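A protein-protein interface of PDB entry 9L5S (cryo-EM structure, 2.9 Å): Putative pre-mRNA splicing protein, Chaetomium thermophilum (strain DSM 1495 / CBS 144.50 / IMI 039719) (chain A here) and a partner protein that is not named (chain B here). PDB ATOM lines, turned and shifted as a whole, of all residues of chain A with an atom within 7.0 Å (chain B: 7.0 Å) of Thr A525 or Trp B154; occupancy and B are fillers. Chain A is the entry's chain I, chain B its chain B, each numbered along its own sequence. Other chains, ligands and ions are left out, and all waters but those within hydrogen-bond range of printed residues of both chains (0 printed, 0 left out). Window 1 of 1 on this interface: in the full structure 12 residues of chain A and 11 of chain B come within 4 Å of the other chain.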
ATOM      1  N   ARG A 522      16.281  -6.675   5.161  1.00  0.00           N
ATOM      2  CA  ARG A 522      17.444  -5.785   5.274  1.00  0.00           C
ATOM      3  C   ARG A 522      17.655  -5.304   6.709  1.00  0.00           C
ATOM      4  O   ARG A 522      18.029  -4.154   6.951  1.00  0.00           O
ATOM      5  CB  ARG A 522      17.341  -4.599   4.310  1.00  0.00           C
ATOM      6  N   ILE A 523      17.414  -6.191   7.669  1.00  0.00           N
ATOM      7  CA  ILE A 523      17.598  -5.892   9.081  1.00  0.00           C
ATOM      8  C   ILE A 523      18.747  -6.705   9.673  1.00  0.00           C
ATOM      9  O   ILE A 523      18.804  -6.906  10.885  1.00  0.00           O
ATOM     10  CB  ILE A 523      16.297  -6.106   9.871  1.00  0.00           C
ATOM     11  N   ALA A 524      19.664  -7.176   8.833  1.00  0.00           N
ATOM     12  CA  ALA A 524      20.791  -7.987   9.272  1.00  0.00           C
ATOM     13  C   ALA A 524      22.045  -7.126   9.343  1.00  0.00           C
ATOM     14  O   ALA A 524      22.425  -6.491   8.355  1.00  0.00           O
ATOM     15  CB  ALA A 524      21.012  -9.169   8.329  1.00  0.00           C
ATOM     16  N   THR A 525      22.685  -7.114  10.509  1.00  0.00           N
ATOM     17  CA  THR A 525      23.897  -6.335  10.718  1.00  0.00           C
ATOM     18  C   THR A 525      25.116  -7.130  10.265  1.00  0.00           C
ATOM     19  O   THR A 525      24.975  -8.268   9.799  1.00  0.00           O
ATOM     20  CB  THR A 525      24.041  -5.941  12.189  1.00  0.00           C
ATOM     21  N   PRO A 526      26.319  -6.555  10.356  1.00  0.00           N
ATOM     22  CA  PRO A 526      27.529  -7.354  10.093  1.00  0.00           C
ATOM     23  C   PRO A 526      27.710  -8.501  11.073  1.00  0.00           C
ATOM     24  O   PRO A 526      28.283  -9.535  10.705  1.00  0.00           O
ATOM     25  CB  PRO A 526      28.659  -6.323  10.210  1.00  0.00           C
ATOM     26  N   GLN A 527      27.237  -8.344  12.312  1.00  0.00           N
ATOM     27  CA  GLN A 527      27.261  -9.448  13.266  1.00  0.00           C
ATOM     28  C   GLN A 527      26.339 -10.576  12.822  1.00  0.00           C
ATOM     29  O   GLN A 527      26.645 -11.755  13.032  1.00  0.00           O
ATOM     30  CB  GLN A 527      26.870  -8.948  14.657  1.00  0.00           C
ATOM     31  N   THR A 528      25.206 -10.235  12.200  1.00  0.00           N
ATOM     32  CA  THR A 528      24.313 -11.259  11.664  1.00  0.00           C
ATOM     33  C   THR A 528      24.965 -12.014  10.511  1.00  0.00           C
ATOM     34  O   THR A 528      24.811 -13.237  10.393  1.00  0.00           O
ATOM     35  CB  THR A 528      22.997 -10.627  11.212  1.00  0.00           C
ATOM     36  N   VAL A 529      25.706 -11.305   9.657  1.00  0.00           N
ATOM     37  CA  VAL A 529      26.420 -11.959   8.563  1.00  0.00           C
ATOM     38  C   VAL A 529      27.536 -12.845   9.103  1.00  0.00           C
ATOM     39  O   VAL A 529      27.793 -13.934   8.575  1.00  0.00           O
ATOM     40  CB  VAL A 529      26.957 -10.909   7.573  1.00  0.00           C
ATOM     41  N   VAL A 530      28.211 -12.396  10.164  1.00  0.00           N
ATOM     42  CA  VAL A 530      29.250 -13.208  10.793  1.00  0.00           C
ATOM     43  C   VAL A 530      28.648 -14.459  11.424  1.00  0.00           C
ATOM     44  O   VAL A 530      29.234 -15.546  11.359  1.00  0.00           O
ATOM     45  CB  VAL A 530      30.030 -12.372  11.824  1.00  0.00           C
ATOM     46  N   ASN A 531      27.473 -14.325  12.045  1.00  0.00           N
ATOM     47  CA  ASN A 531      26.787 -15.481  12.617  1.00  0.00           C
ATOM     48  C   ASN A 531      26.343 -16.458  11.534  1.00  0.00           C
ATOM     49  O   ASN A 531      26.421 -17.676  11.723  1.00  0.00           O
ATOM     50  CB  ASN A 531      25.590 -15.021  13.449  1.00  0.00           C
ATOM     51  N   GLY A 552      27.882  -9.806   2.927  1.00  0.00           N
ATOM     52  CA  GLY A 552      28.208  -8.759   3.884  1.00  0.00           C
ATOM     53  C   GLY A 552      29.026  -7.639   3.271  1.00  0.00           C
ATOM     54  O   GLY A 552      28.851  -6.468   3.617  1.00  0.00           O
ATOM     55  N   PHE A 556      27.114  -3.639   2.599  1.00  0.00           N
ATOM     56  CA  PHE A 556      27.737  -2.437   3.141  1.00  0.00           C
ATOM     57  C   PHE A 556      29.184  -2.412   2.674  1.00  0.00           C
ATOM     58  O   PHE A 556      29.984  -3.249   3.098  1.00  0.00           O
ATOM     59  CB  PHE A 556      27.656  -2.410   4.668  1.00  0.00           C
ATOM     60  N   VAL A 560      31.528  -0.596   6.947  1.00  0.00           N
ATOM     61  CA  VAL A 560      30.899  -1.586   7.822  1.00  0.00           C
ATOM     62  C   VAL A 560      31.276  -3.018   7.487  1.00  0.00           C
ATOM     63  O   VAL A 560      30.765  -3.943   8.132  1.00  0.00           O
ATOM     64  CB  VAL A 560      29.364  -1.449   7.789  1.00  0.00           C
ATOM     65  N   GLU B 147      34.357   5.220  15.806  1.00  0.00           N
ATOM     66  CA  GLU B 147      33.548   5.065  14.602  1.00  0.00           C
ATOM     67  C   GLU B 147      33.507   3.611  14.141  1.00  0.00           C
ATOM     68  O   GLU B 147      32.462   3.131  13.692  1.00  0.00           O
ATOM     69  CB  GLU B 147      34.060   6.004  13.501  1.00  0.00           C
ATOM     70  CG  GLU B 147      35.502   5.794  13.023  1.00  0.00           C
ATOM     71  CD  GLU B 147      35.632   4.747  11.929  1.00  0.00           C
ATOM     72  OE1 GLU B 147      34.617   4.442  11.268  1.00  0.00           O
ATOM     73  OE2 GLU B 147      36.751   4.225  11.734  1.00  0.00           O
ATOM     74  N   ARG B 148      34.617   2.878  14.282  1.00  0.00           N
ATOM     75  CA  ARG B 148      34.605   1.453  13.958  1.00  0.00           C
ATOM     76  C   ARG B 148      33.780   0.656  14.961  1.00  0.00           C
ATOM     77  O   ARG B 148      33.103  -0.310  14.581  1.00  0.00           O
ATOM     78  CB  ARG B 148      36.034   0.917  13.898  1.00  0.00           C
ATOM     79  CG  ARG B 148      36.165  -0.481  13.313  1.00  0.00           C
ATOM     80  CD  ARG B 148      37.623  -0.820  13.038  1.00  0.00           C
ATOM     81  NE  ARG B 148      37.778  -2.115  12.386  1.00  0.00           N
ATOM     82  CZ  ARG B 148      38.937  -2.609  11.969  1.00  0.00           C
ATOM     83  NH1 ARG B 148      40.067  -1.936  12.113  1.00  0.00           N
ATOM     84  NH2 ARG B 148      38.961  -3.806  11.389  1.00  0.00           N
ATOM     85  N   LYS B 149      33.822   1.051  16.239  1.00  0.00           N
ATOM     86  CA  LYS B 149      33.004   0.404  17.261  1.00  0.00           C
ATOM     87  C   LYS B 149      31.519   0.581  16.971  1.00  0.00           C
ATOM     88  O   LYS B 149      30.724  -0.337  17.205  1.00  0.00           O
ATOM     89  CB  LYS B 149      33.353   0.953  18.643  1.00  0.00           C
ATOM     90  CG  LYS B 149      34.790   0.706  19.065  1.00  0.00           C
ATOM     91  CD  LYS B 149      35.055  -0.778  19.266  1.00  0.00           C
ATOM     92  CE  LYS B 149      36.472  -1.030  19.757  1.00  0.00           C
ATOM     93  NZ  LYS B 149      36.752  -2.484  19.912  1.00  0.00           N
ATOM     94  N   ARG B 150      31.123   1.755  16.474  1.00  0.00           N
ATOM     95  CA  ARG B 150      29.762   1.888  15.964  1.00  0.00           C
ATOM     96  C   ARG B 150      29.561   1.069  14.694  1.00  0.00           C
ATOM     97  O   ARG B 150      28.489   0.486  14.499  1.00  0.00           O
ATOM     98  CB  ARG B 150      29.423   3.355  15.701  1.00  0.00           C
ATOM     99  CG  ARG B 150      29.369   4.217  16.946  1.00  0.00           C
ATOM    100  CD  ARG B 150      28.961   5.642  16.611  1.00  0.00           C
ATOM    101  NE  ARG B 150      27.511   5.799  16.573  1.00  0.00           N
ATOM    102  CZ  ARG B 150      26.887   6.924  16.254  1.00  0.00           C
ATOM    103  NH1 ARG B 150      27.557   8.019  15.933  1.00  0.00           N
ATOM    104  NH2 ARG B 150      25.557   6.953  16.263  1.00  0.00           N
ATOM    105  N   ALA B 151      30.584   0.994  13.836  1.00  0.00           N
ATOM    106  CA  ALA B 151      30.483   0.336  12.539  1.00  0.00           C
ATOM    107  C   ALA B 151      30.406  -1.180  12.632  1.00  0.00           C
ATOM    108  O   ALA B 151      30.154  -1.828  11.610  1.00  0.00           O
ATOM    109  CB  ALA B 151      31.670   0.733  11.659  1.00  0.00           C
ATOM    110  N   TRP B 152      30.637  -1.759  13.812  1.00  0.00           N
ATOM    111  CA  TRP B 152      30.445  -3.199  13.969  1.00  0.00           C
ATOM    112  C   TRP B 152      28.992  -3.622  13.764  1.00  0.00           C
ATOM    113  O   TRP B 152      28.741  -4.674  13.166  1.00  0.00           O
ATOM    114  CB  TRP B 152      30.923  -3.662  15.348  1.00  0.00           C
ATOM    115  CG  TRP B 152      32.410  -3.773  15.491  1.00  0.00           C
ATOM    116  CD1 TRP B 152      33.232  -2.939  16.188  1.00  0.00           C
ATOM    117  CD2 TRP B 152      33.249  -4.796  14.940  1.00  0.00           C
ATOM    118  NE1 TRP B 152      34.534  -3.370  16.095  1.00  0.00           N
ATOM    119  CE2 TRP B 152      34.570  -4.509  15.335  1.00  0.00           C
ATOM    120  CE3 TRP B 152      33.012  -5.922  14.145  1.00  0.00           C
ATOM    121  CZ2 TRP B 152      35.651  -5.308  14.965  1.00  0.00           C
ATOM    122  CZ3 TRP B 152      34.085  -6.714  13.779  1.00  0.00           C
ATOM    123  CH2 TRP B 152      35.388  -6.403  14.190  1.00  0.00           C
ATOM    124  N   ASP B 153      28.029  -2.836  14.242  1.00  0.00           N
ATOM    125  CA  ASP B 153      26.655  -3.319  14.374  1.00  0.00           C
ATOM    126  C   ASP B 153      25.630  -2.303  13.865  1.00  0.00           C
ATOM    127  O   ASP B 153      24.664  -1.968  14.554  1.00  0.00           O
ATOM    128  CB  ASP B 153      26.363  -3.694  15.826  1.00  0.00           C
ATOM    129  CG  ASP B 153      26.829  -2.636  16.807  1.00  0.00           C
ATOM    130  OD1 ASP B 153      27.554  -1.710  16.386  1.00  0.00           O
ATOM    131  OD2 ASP B 153      26.470  -2.731  17.999  1.00  0.00           O
ATOM    132  N   TRP B 154      25.817  -1.794  12.648  1.00  0.00           N
ATOM    133  CA  TRP B 154      24.738  -1.067  11.990  1.00  0.00           C
ATOM    134  C   TRP B 154      23.910  -2.005  11.121  1.00  0.00           C
ATOM    135  O   TRP B 154      24.402  -3.017  10.615  1.00  0.00           O
ATOM    136  CB  TRP B 154      25.245   0.081  11.115  1.00  0.00           C
ATOM    137  CG  TRP B 154      25.958   1.165  11.841  1.00  0.00           C
ATOM    138  CD1 TRP B 154      27.293   1.404  11.836  1.00  0.00           C
ATOM    139  CD2 TRP B 154      25.374   2.149  12.701  1.00  0.00           C
ATOM    140  NE1 TRP B 154      27.585   2.488  12.629  1.00  0.00           N
ATOM    141  CE2 TRP B 154      26.422   2.961  13.175  1.00  0.00           C
ATOM    142  CE3 TRP B 154      24.068   2.425  13.114  1.00  0.00           C
ATOM    143  CZ2 TRP B 154      26.206   4.031  14.039  1.00  0.00           C
ATOM    144  CZ3 TRP B 154      23.854   3.487  13.973  1.00  0.00           C
ATOM    145  CH2 TRP B 154      24.917   4.276  14.428  1.00  0.00           C
ATOM    146  N   THR B 155      22.641  -1.649  10.945  1.00  0.00           N
ATOM    147  CA  THR B 155      21.787  -2.343   9.997  1.00  0.00           C
ATOM    148  C   THR B 155      22.088  -1.867   8.576  1.00  0.00           C
ATOM    149  O   THR B 155      22.871  -0.938   8.354  1.00  0.00           O
ATOM    150  CB  THR B 155      20.311  -2.125  10.335  1.00  0.00           C
ATOM    151  OG1 THR B 155      19.495  -2.827   9.389  1.00  0.00           O
ATOM    152  CG2 THR B 155      19.966  -0.646  10.293  1.00  0.00           C
ATOM    153  N   VAL B 156      21.462  -2.533   7.604  1.00  0.00           N
ATOM    154  CA  VAL B 156      21.717  -2.219   6.199  1.00  0.00           C
ATOM    155  C   VAL B 156      21.154  -0.848   5.841  1.00  0.00           C
ATOM    156  O   VAL B 156      21.860   0.000   5.278  1.00  0.00           O
ATOM    157  CB  VAL B 156      21.135  -3.320   5.296  1.00  0.00           C
ATOM    158  CG1 VAL B 156      21.366  -2.988   3.835  1.00  0.00           C
ATOM    159  CG2 VAL B 156      21.745  -4.669   5.643  1.00  0.00           C
ATOM    160  N   GLU B 157      19.888  -0.600   6.207  1.00  0.00           N
ATOM    161  CA  GLU B 157      19.187   0.615   5.792  1.00  0.00           C
ATOM    162  C   GLU B 157      19.876   1.865   6.321  1.00  0.00           C
ATOM    163  O   GLU B 157      19.955   2.883   5.621  1.00  0.00           O
ATOM    164  CB  GLU B 157      17.735   0.565   6.267  1.00  0.00           C
ATOM    165  CG  GLU B 157      16.873  -0.448   5.533  1.00  0.00           C
ATOM    166  CD  GLU B 157      15.393  -0.246   5.792  1.00  0.00           C
ATOM    167  OE1 GLU B 157      14.969   0.917   5.953  1.00  0.00           O
ATOM    168  OE2 GLU B 157      14.654  -1.253   5.835  1.00  0.00           O
ATOM    169  N   GLU B 158      20.408   1.794   7.544  1.00  0.00           N
ATOM    170  CA  GLU B 158      21.224   2.882   8.063  1.00  0.00           C
ATOM    171  C   GLU B 158      22.496   3.068   7.246  1.00  0.00           C
ATOM    172  O   GLU B 158      22.969   4.198   7.092  1.00  0.00           O
ATOM    173  CB  GLU B 158      21.569   2.625   9.530  1.00  0.00           C
ATOM    174  CG  GLU B 158      21.948   3.873  10.306  1.00  0.00           C
ATOM    175  CD  GLU B 158      20.749   4.739  10.638  1.00  0.00           C
ATOM    176  OE1 GLU B 158      19.633   4.191  10.756  1.00  0.00           O
ATOM    177  OE2 GLU B 158      20.922   5.967  10.781  1.00  0.00           O
ATOM    178  N   ALA B 159      23.053   1.981   6.699  1.00  0.00           N
ATOM    179  CA  ALA B 159      24.262   2.111   5.891  1.00  0.00           C
ATOM    180  C   ALA B 159      23.980   2.810   4.565  1.00  0.00           C
ATOM    181  O   ALA B 159      24.745   3.698   4.165  1.00  0.00           O
ATOM    182  CB  ALA B 159      24.914   0.746   5.663  1.00  0.00           C
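O of Arg A522 sits at hydrogen-bond distance from OG1 of Thr B155, at 3.1 Å.
O of Arg B150 is in hydrogen-bond range of NE1 of Trp B154 (2.9 Å).
Among the printed residues, merely in contact across the chains: Ala A524 with Val B156 (3.3 Å), Thr A525 with Trp B154 (3.3 Å), Pro A526 with Trp B152 (3.4 Å), Arg A522 with Val B156 (3.6 Å), Ile A523 with Thr B155 (3.6 Å) and Val A560 with Ala B151 (3.9 Å).
Printed residues of chain B within 4 Å of Ile A523: Thr B155.
Thr A525 touches one residue of chain B.
Of the printed residues of chain B, Pro A526 touches Trp B152 (3.4 Å).
Of the printed residues of chain A, Ala B151 touches Val A560.
Trp B154 touches just one residue of chain A: Thr A525.
The nearest residue of chain A that does not touch Trp B154 is Pro A526 (4.03 Å).
Hydrophobic or aromatic side chains of chain A that line the printed part of chain B: Pro A526 and Val A560.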
